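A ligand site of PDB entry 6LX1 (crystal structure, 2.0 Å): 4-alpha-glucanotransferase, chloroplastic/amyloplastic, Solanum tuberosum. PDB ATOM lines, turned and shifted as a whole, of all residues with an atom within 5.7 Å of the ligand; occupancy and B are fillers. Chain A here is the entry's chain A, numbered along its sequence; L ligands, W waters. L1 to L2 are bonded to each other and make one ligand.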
ATOM      1  N   SER A  82      -4.443 -19.064 -20.083  1.00  0.00           N
ATOM      2  CA  SER A  82      -4.769 -19.729 -18.792  1.00  0.00           C
ATOM      3  C   SER A  82      -6.248 -19.569 -18.481  1.00  0.00           C
ATOM      4  O   SER A  82      -6.702 -18.449 -18.233  1.00  0.00           O
ATOM      5  CB  SER A  82      -3.987 -19.201 -17.632  1.00  0.00           C
ATOM      6  OG  SER A  82      -4.396 -19.897 -16.472  1.00  0.00           O
ATOM      7  N   TYR A  84      -7.406 -20.149 -15.668  1.00  0.00           N
ATOM      8  CA  TYR A  84      -7.407 -19.815 -14.214  1.00  0.00           C
ATOM      9  C   TYR A  84      -6.985 -18.370 -13.949  1.00  0.00           C
ATOM     10  O   TYR A  84      -7.081 -17.999 -12.793  1.00  0.00           O
ATOM     11  CB  TYR A  84      -6.581 -20.854 -13.429  1.00  0.00           C
ATOM     12  CG  TYR A  84      -7.203 -22.231 -13.533  1.00  0.00           C
ATOM     13  CD1 TYR A  84      -8.214 -22.647 -12.703  1.00  0.00           C
ATOM     14  CD2 TYR A  84      -6.785 -23.105 -14.532  1.00  0.00           C
ATOM     15  CE1 TYR A  84      -8.799 -23.906 -12.846  1.00  0.00           C
ATOM     16  CE2 TYR A  84      -7.368 -24.355 -14.696  1.00  0.00           C
ATOM     17  CZ  TYR A  84      -8.390 -24.744 -13.852  1.00  0.00           C
ATOM     18  OH  TYR A  84      -8.928 -25.994 -14.040  1.00  0.00           O
ATOM     19  N   SER A  85      -6.726 -17.587 -14.983  1.00  0.00           N
ATOM     20  CA  SER A  85      -6.344 -16.155 -14.937  1.00  0.00           C
ATOM     21  C   SER A  85      -7.364 -15.372 -15.756  1.00  0.00           C
ATOM     22  O   SER A  85      -6.974 -14.663 -16.669  1.00  0.00           O
ATOM     23  CB  SER A  85      -4.943 -15.967 -15.531  1.00  0.00           C
ATOM     24  OG  SER A  85      -4.050 -16.682 -14.759  1.00  0.00           O
ATOM     25  N   ASP A 241     -15.393 -26.016 -13.409  1.00  0.00           N
ATOM     26  CA  ASP A 241     -14.298 -25.740 -12.466  1.00  0.00           C
ATOM     27  C   ASP A 241     -14.276 -24.237 -12.232  1.00  0.00           C
ATOM     28  O   ASP A 241     -14.604 -23.478 -13.138  1.00  0.00           O
ATOM     29  CB  ASP A 241     -12.961 -26.207 -13.045  1.00  0.00           C
ATOM     30  CG  ASP A 241     -11.839 -26.418 -12.053  1.00  0.00           C
ATOM     31  OD1 ASP A 241     -12.054 -26.237 -10.807  1.00  0.00           O
ATOM     32  OD2 ASP A 241     -10.726 -26.780 -12.540  1.00  0.00           O
ATOM     33  N   PRO A 243     -11.827 -21.154  -9.958  1.00  0.00           N
ATOM     34  CA  PRO A 243     -10.827 -20.813  -8.935  1.00  0.00           C
ATOM     35  C   PRO A 243     -11.629 -20.225  -7.761  1.00  0.00           C
ATOM     36  O   PRO A 243     -12.618 -19.508  -8.007  1.00  0.00           O
ATOM     37  CB  PRO A 243      -9.871 -19.846  -9.669  1.00  0.00           C
ATOM     38  CG  PRO A 243     -10.722 -19.255 -10.793  1.00  0.00           C
ATOM     39  CD  PRO A 243     -11.731 -20.323 -11.185  1.00  0.00           C
ATOM     40  N   GLN A 284       4.504 -19.592  -2.238  1.00  0.00           N
ATOM     41  CA  GLN A 284       3.856 -19.202  -3.535  1.00  0.00           C
ATOM     42  C   GLN A 284       2.983 -17.943  -3.309  1.00  0.00           C
ATOM     43  O   GLN A 284       2.020 -17.989  -2.487  1.00  0.00           O
ATOM     44  CB  GLN A 284       3.107 -20.417  -4.076  1.00  0.00           C
ATOM     45  CG  GLN A 284       3.000 -20.491  -5.600  1.00  0.00           C
ATOM     46  CD  GLN A 284       2.264 -21.731  -6.058  1.00  0.00           C
ATOM     47  OE1 GLN A 284       2.058 -22.676  -5.303  1.00  0.00           O
ATOM     48  NE2 GLN A 284       1.818 -21.737  -7.306  1.00  0.00           N
ATOM     49  N   LEU A 285       3.336 -16.822  -3.956  1.00  0.00           N
ATOM     50  CA  LEU A 285       2.554 -15.562  -3.956  1.00  0.00           C
ATOM     51  C   LEU A 285       1.615 -15.575  -5.163  1.00  0.00           C
ATOM     52  O   LEU A 285       2.121 -15.329  -6.259  1.00  0.00           O
ATOM     53  CB  LEU A 285       3.489 -14.350  -4.017  1.00  0.00           C
ATOM     54  CG  LEU A 285       2.789 -12.992  -4.044  1.00  0.00           C
ATOM     55  CD1 LEU A 285       2.051 -12.744  -2.739  1.00  0.00           C
ATOM     56  CD2 LEU A 285       3.774 -11.861  -4.312  1.00  0.00           C
ATOM     57  N   TRP A 286       0.322 -15.821  -4.986  1.00  0.00           N
ATOM     58  CA  TRP A 286      -0.660 -15.853  -6.105  1.00  0.00           C
ATOM     59  C   TRP A 286      -1.137 -14.446  -6.439  1.00  0.00           C
ATOM     60  O   TRP A 286      -1.304 -14.197  -7.606  1.00  0.00           O
ATOM     61  CB  TRP A 286      -1.863 -16.734  -5.821  1.00  0.00           C
ATOM     62  CG  TRP A 286      -1.531 -18.166  -5.598  1.00  0.00           C
ATOM     63  CD1 TRP A 286      -0.425 -18.852  -6.033  1.00  0.00           C
ATOM     64  CD2 TRP A 286      -2.356 -19.105  -4.897  1.00  0.00           C
ATOM     65  NE1 TRP A 286      -0.502 -20.159  -5.616  1.00  0.00           N
ATOM     66  CE2 TRP A 286      -1.675 -20.347  -4.926  1.00  0.00           C
ATOM     67  CE3 TRP A 286      -3.583 -19.005  -4.236  1.00  0.00           C
ATOM     68  CZ2 TRP A 286      -2.197 -21.476  -4.315  1.00  0.00           C
ATOM     69  CZ3 TRP A 286      -4.100 -20.132  -3.638  1.00  0.00           C
ATOM     70  CH2 TRP A 286      -3.399 -21.345  -3.673  1.00  0.00           C
ATOM     71  N   ARG A 319     -16.036 -28.354  -9.755  1.00  0.00           N
ATOM     72  CA  ARG A 319     -14.941 -28.308  -8.772  1.00  0.00           C
ATOM     73  C   ARG A 319     -14.752 -26.862  -8.302  1.00  0.00           C
ATOM     74  O   ARG A 319     -14.922 -25.945  -9.103  1.00  0.00           O
ATOM     75  CB  ARG A 319     -13.666 -28.836  -9.418  1.00  0.00           C
ATOM     76  CG  ARG A 319     -12.551 -29.110  -8.426  1.00  0.00           C
ATOM     77  CD  ARG A 319     -11.344 -29.673  -9.168  1.00  0.00           C
ATOM     78  NE  ARG A 319     -10.602 -28.583  -9.770  1.00  0.00           N
ATOM     79  CZ  ARG A 319      -9.270 -28.544  -9.923  1.00  0.00           C
ATOM     80  NH1 ARG A 319      -8.517 -29.579  -9.580  1.00  0.00           N
ATOM     81  NH2 ARG A 319      -8.672 -27.477 -10.458  1.00  0.00           N
ATOM     82  N   ASP A 321     -11.504 -24.938  -7.057  1.00  0.00           N
ATOM     83  CA  ASP A 321     -10.031 -25.029  -6.869  1.00  0.00           C
ATOM     84  C   ASP A 321      -9.645 -24.227  -5.618  1.00  0.00           C
ATOM     85  O   ASP A 321     -10.093 -23.087  -5.463  1.00  0.00           O
ATOM     86  CB  ASP A 321      -9.415 -24.570  -8.181  1.00  0.00           C
ATOM     87  CG  ASP A 321      -7.932 -24.793  -8.385  1.00  0.00           C
ATOM     88  OD1 ASP A 321      -7.275 -25.264  -7.463  1.00  0.00           O
ATOM     89  OD2 ASP A 321      -7.475 -24.584  -9.557  1.00  0.00           O
ATOM     90  N   GLU A 368     -11.628 -29.407  -4.336  1.00  0.00           N
ATOM     91  CA  GLU A 368     -10.189 -29.649  -4.629  1.00  0.00           C
ATOM     92  C   GLU A 368      -9.475 -29.560  -3.274  1.00  0.00           C
ATOM     93  O   GLU A 368      -9.495 -28.486  -2.651  1.00  0.00           O
ATOM     94  CB  GLU A 368      -9.613 -28.643  -5.633  1.00  0.00           C
ATOM     95  CG  GLU A 368      -8.122 -28.846  -5.863  1.00  0.00           C
ATOM     96  CD  GLU A 368      -7.179 -28.158  -4.857  1.00  0.00           C
ATOM     97  OE1 GLU A 368      -7.231 -26.903  -4.732  1.00  0.00           O
ATOM     98  OE2 GLU A 368      -6.312 -28.857  -4.254  1.00  0.00           O
ATOM     99  N   HIS A 420      -5.415 -31.929 -15.296  1.00  0.00           N
ATOM    100  CA  HIS A 420      -4.729 -31.035 -16.263  1.00  0.00           C
ATOM    101  C   HIS A 420      -3.398 -30.507 -15.681  1.00  0.00           C
ATOM    102  O   HIS A 420      -2.593 -30.032 -16.493  1.00  0.00           O
ATOM    103  CB  HIS A 420      -5.666 -29.866 -16.648  1.00  0.00           C
ATOM    104  CG  HIS A 420      -6.031 -29.082 -15.456  1.00  0.00           C
ATOM    105  ND1 HIS A 420      -7.039 -29.485 -14.587  1.00  0.00           N
ATOM    106  CD2 HIS A 420      -5.469 -27.975 -14.926  1.00  0.00           C
ATOM    107  CE1 HIS A 420      -7.093 -28.622 -13.615  1.00  0.00           C
ATOM    108  NE2 HIS A 420      -6.117 -27.735 -13.758  1.00  0.00           N
ATOM    109  N   ASP A 421      -3.211 -30.528 -14.357  1.00  0.00           N
ATOM    110  CA  ASP A 421      -1.956 -30.113 -13.666  1.00  0.00           C
ATOM    111  C   ASP A 421      -0.910 -31.240 -13.637  1.00  0.00           C
ATOM    112  O   ASP A 421       0.278 -30.975 -13.297  1.00  0.00           O
ATOM    113  CB  ASP A 421      -2.249 -29.596 -12.253  1.00  0.00           C
ATOM    114  CG  ASP A 421      -2.927 -28.224 -12.190  1.00  0.00           C
ATOM    115  OD1 ASP A 421      -2.760 -27.449 -13.157  1.00  0.00           O
ATOM    116  OD2 ASP A 421      -3.713 -27.991 -11.256  1.00  0.00           O
ATOM    117  N   ASN A 485      -0.847 -28.596 -18.597  1.00  0.00           N
ATOM    118  CA  ASN A 485      -0.246 -27.557 -17.728  1.00  0.00           C
ATOM    119  C   ASN A 485       0.904 -28.169 -16.924  1.00  0.00           C
ATOM    120  O   ASN A 485       0.733 -29.271 -16.371  1.00  0.00           O
ATOM    121  CB  ASN A 485      -1.254 -26.917 -16.774  1.00  0.00           C
ATOM    122  CG  ASN A 485      -0.691 -25.798 -15.947  1.00  0.00           C
ATOM    123  OD1 ASN A 485      -0.072 -24.887 -16.503  1.00  0.00           O
ATOM    124  ND2 ASN A 485      -0.911 -25.806 -14.652  1.00  0.00           N
ATOM    125  N   ILE A 486       2.025 -27.444 -16.824  1.00  0.00           N
ATOM    126  CA  ILE A 486       3.066 -27.674 -15.776  1.00  0.00           C
ATOM    127  C   ILE A 486       2.920 -26.564 -14.752  1.00  0.00           C
ATOM    128  O   ILE A 486       3.204 -25.399 -15.030  1.00  0.00           O
ATOM    129  CB  ILE A 486       4.497 -27.736 -16.382  1.00  0.00           C
ATOM    130  CG1 ILE A 486       4.603 -28.748 -17.514  1.00  0.00           C
ATOM    131  CG2 ILE A 486       5.491 -28.013 -15.256  1.00  0.00           C
ATOM    132  CD1 ILE A 486       5.928 -28.749 -18.286  1.00  0.00           C
ATOM    133  N   PRO A 487       2.406 -26.820 -13.541  1.00  0.00           N
ATOM    134  CA  PRO A 487       2.217 -25.749 -12.569  1.00  0.00           C
ATOM    135  C   PRO A 487       3.430 -24.813 -12.343  1.00  0.00           C
ATOM    136  O   PRO A 487       4.528 -25.300 -12.231  1.00  0.00           O
ATOM    137  CB  PRO A 487       1.892 -26.517 -11.302  1.00  0.00           C
ATOM    138  CG  PRO A 487       1.156 -27.747 -11.819  1.00  0.00           C
ATOM    139  CD  PRO A 487       1.897 -28.121 -13.074  1.00  0.00           C
ATOM    140  N   ALA A 488       3.162 -23.513 -12.359  1.00  0.00           N
ATOM    141  CA  ALA A 488       4.110 -22.373 -12.216  1.00  0.00           C
ATOM    142  C   ALA A 488       4.913 -22.103 -13.495  1.00  0.00           C
ATOM    143  O   ALA A 488       5.552 -21.039 -13.538  1.00  0.00           O
ATOM    144  CB  ALA A 488       4.994 -22.560 -11.011  1.00  0.00           C
ATOM    145  N   THR A 489       4.907 -22.934 -14.534  1.00  0.00           N
ATOM    146  CA  THR A 489       5.694 -22.611 -15.762  1.00  0.00           C
ATOM    147  C   THR A 489       4.962 -21.543 -16.584  1.00  0.00           C
ATOM    148  O   THR A 489       3.754 -21.312 -16.328  1.00  0.00           O
ATOM    149  CB  THR A 489       5.999 -23.849 -16.611  1.00  0.00           C
ATOM    150  OG1 THR A 489       4.792 -24.343 -17.220  1.00  0.00           O
ATOM    151  CG2 THR A 489       6.699 -24.894 -15.775  1.00  0.00           C
ATOM    152  N   GLN A 490       5.652 -20.884 -17.517  1.00  0.00           N
ATOM    153  CA  GLN A 490       5.069 -19.711 -18.212  1.00  0.00           C
ATOM    154  C   GLN A 490       4.748 -20.044 -19.672  1.00  0.00           C
ATOM    155  O   GLN A 490       4.050 -19.255 -20.247  1.00  0.00           O
ATOM    156  CB  GLN A 490       5.996 -18.501 -18.069  1.00  0.00           C
ATOM    157  CG  GLN A 490       6.069 -17.975 -16.652  1.00  0.00           C
ATOM    158  CD  GLN A 490       4.700 -17.955 -16.002  1.00  0.00           C
ATOM    159  OE1 GLN A 490       3.912 -17.035 -16.208  1.00  0.00           O
ATOM    160  NE2 GLN A 490       4.401 -18.997 -15.229  1.00  0.00           N
ATOM    161  N   TRP A 494      -1.745 -25.016 -21.750  1.00  0.00           N
ATOM    162  CA  TRP A 494      -3.158 -24.856 -22.203  1.00  0.00           C
ATOM    163  C   TRP A 494      -3.291 -24.953 -23.714  1.00  0.00           C
ATOM    164  O   TRP A 494      -4.344 -24.566 -24.198  1.00  0.00           O
ATOM    165  CB  TRP A 494      -3.682 -23.503 -21.690  1.00  0.00           C
ATOM    166  CG  TRP A 494      -3.294 -23.168 -20.285  1.00  0.00           C
ATOM    167  CD1 TRP A 494      -2.508 -22.151 -19.874  1.00  0.00           C
ATOM    168  CD2 TRP A 494      -3.688 -23.868 -19.091  1.00  0.00           C
ATOM    169  NE1 TRP A 494      -2.357 -22.168 -18.523  1.00  0.00           N
ATOM    170  CE2 TRP A 494      -3.070 -23.215 -18.013  1.00  0.00           C
ATOM    171  CE3 TRP A 494      -4.493 -24.982 -18.835  1.00  0.00           C
ATOM    172  CZ2 TRP A 494      -3.245 -23.635 -16.687  1.00  0.00           C
ATOM    173  CZ3 TRP A 494      -4.687 -25.381 -17.528  1.00  0.00           C
ATOM    174  CH2 TRP A 494      -4.086 -24.698 -16.460  1.00  0.00           C
HETATM  175  C1  LIG L   1      -6.036 -24.530  -9.722  1.00  0.00           C
HETATM  176  C2  LIG L   1      -5.730 -25.044 -11.109  1.00  0.00           C
HETATM  177  C3  LIG L   1      -4.309 -24.683 -11.512  1.00  0.00           C
HETATM  178  C4  LIG L   1      -4.110 -23.165 -11.387  1.00  0.00           C
HETATM  179  C5  LIG L   1      -4.405 -22.775  -9.978  1.00  0.00           C
HETATM  180  C6  LIG L   1      -4.073 -21.306  -9.752  1.00  0.00           C
HETATM  181  O1  LIG L   1      -5.929 -26.458 -11.180  1.00  0.00           O
HETATM  182  O2  LIG L   1      -4.045 -25.109 -12.837  1.00  0.00           O
HETATM  183  O3  LIG L   1      -2.736 -22.858 -11.625  1.00  0.00           O
HETATM  184  O4  LIG L   1      -5.776 -23.106  -9.668  1.00  0.00           O
HETATM  185  O5  LIG L   1      -4.887 -20.801  -8.744  1.00  0.00           O
HETATM  186  C1  LG2 L   2      -2.444 -22.552 -12.970  1.00  0.00           C
HETATM  187  O1  LG2 L   2      -0.470 -23.845 -12.476  1.00  0.00           O
HETATM  188  C2  LG2 L   2      -0.930 -22.619 -13.056  1.00  0.00           C
HETATM  189  C3  LG2 L   2       1.267 -15.440 -12.469  1.00  0.00           C
HETATM  190  C4  LG2 L   2      -0.279 -21.415 -12.352  1.00  0.00           C
HETATM  191  O2  LG2 L   2       1.073 -21.463 -12.831  1.00  0.00           O
HETATM  192  C5  LG2 L   2      -0.928 -20.114 -12.849  1.00  0.00           C
HETATM  193  N1  LG2 L   2      -0.258 -18.898 -12.478  1.00  0.00           N
HETATM  194  C6  LG2 L   2      -2.418 -20.113 -12.568  1.00  0.00           C
HETATM  195  O3  LG2 L   2      -2.932 -21.253 -13.316  1.00  0.00           O
HETATM  196  C7  LG2 L   2      -3.132 -18.856 -13.117  1.00  0.00           C
HETATM  197  C8  LG2 L   2       0.100 -17.933 -13.564  1.00  0.00           C
HETATM  198  C9  LG2 L   2       1.595 -17.658 -13.517  1.00  0.00           C
HETATM  199  O4  LG2 L   2       2.279 -18.922 -13.621  1.00  0.00           O
HETATM  200  C10 LG2 L   2       1.828 -16.829 -12.234  1.00  0.00           C
HETATM  201  O5  LG2 L   2       3.216 -16.672 -11.874  1.00  0.00           O
HETATM  202  O6  LG2 L   2       1.201 -14.845 -11.175  1.00  0.00           O
HETATM  203  C11 LG2 L   2      -0.082 -15.449 -13.183  1.00  0.00           C
HETATM  204  C12 LG2 L   2      -0.622 -16.603 -13.651  1.00  0.00           C
HETATM  205  C13 LG2 L   2      -0.801 -14.136 -13.463  1.00  0.00           C
HETATM  206  O7  LG2 L   2      -1.818 -13.875 -12.490  1.00  0.00           O
HETATM  207  O   HOH W   1      -0.826 -19.175  -9.533  1.00  0.00           O
HETATM  208  O   HOH W   2      -7.556 -21.465  -7.327  1.00  0.00           O
HETATM  209  O   HOH W   3       1.172 -22.672 -15.756  1.00  0.00           O
HETATM  210  O   HOH W   4      -0.564 -24.204  -9.849  1.00  0.00           O
HETATM  211  O   HOH W   5      -4.116 -18.281  -8.458  1.00  0.00           O
HETATM  212  O   HOH W   6      -1.517 -20.357 -15.961  1.00  0.00           O
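Merely in contact with the ligand: Ser 85 (2.9 Å), Pro 487 (3.3 Å), Trp 494 (3.6 Å), Tyr 84 (3.7 Å), Ser 82 (3.7 Å) and Thr 489 (3.9 Å).
Hydrophobic or aromatic side chains within 4 Å of the ligand: Tyr 84, His 420, Pro 487 and Trp 494.
Of the 20 residues printed, 13 come within 4 Å of the ligand.
The nearest printed residue that does not touch the ligand is Trp 286 (4.4 Å).
OD2 of Asp 321 is bonded to C1 of LIG L1 (1.4 Å).
An oxygen (O4) of LG2 L2 sits at hydrogen-bond distance from the side-chain amide nitrogen (NE2) of Gln 490 (2.7 Å).
The side-chain carboxylate (OD1) of Asp 421 lies within hydrogen-bond range of an oxygen (O2) of LIG L1, at 2.7 Å.
An oxygen (O1) of LIG L1 sits at hydrogen-bond distance from a ring nitrogen (NE2) of His 420 (2.9 Å).
The side-chain amide nitrogen (ND2) of Asn 485 is in hydrogen-bond range of an oxygen (O1) of LG2 L2.
An oxygen (O2) of LG2 L2 sits at hydrogen-bond distance from the backbone NH (N) of Ala 488 (3.0 Å).
The guanidinium group (NH2) of Arg 319 sits at hydrogen-bond distance from an oxygen (O1) of LIG L1 (3.0 Å).
Water W6 lies within hydrogen-bond range of the side-chain hydroxyl of Ser 82 (3.0 Å), an oxygen (O3) of LG2 L2 (3.1 Å) and the indole nitrogen of Trp 494 (3.2 Å).
The side-chain carboxylate (OD2) of Asp 321 lies within salt-bridge range of the guanidinium group (NH2) of Arg 319, at 3.3 Å.
NE2 of Gln 490 lies within hydrogen-bond range of O of Ala 488.
OD1 of Asp 421 is in hydrogen-bond range of ND2 of Asn 485 (2.9 Å).
The backbone NH (N) of Asn 485 lies within hydrogen-bond range of the backbone carbonyl oxygen (O) of His 420 (3.1 Å).
NE2 of His 420 lies close to OH of Tyr 84 (3.3 Å).
OD1 of Asp 241 is in salt-bridge range of NE of Arg 319 (2.9 Å).
The backbone NH (N) of Tyr 84 sits close to the side-chain hydroxyl (OG) of Ser 82.
The side-chain hydroxyl (OG1) of Thr 489 sits at hydrogen-bond distance from the backbone carbonyl oxygen (O) of Ile 486 (2.9 Å).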
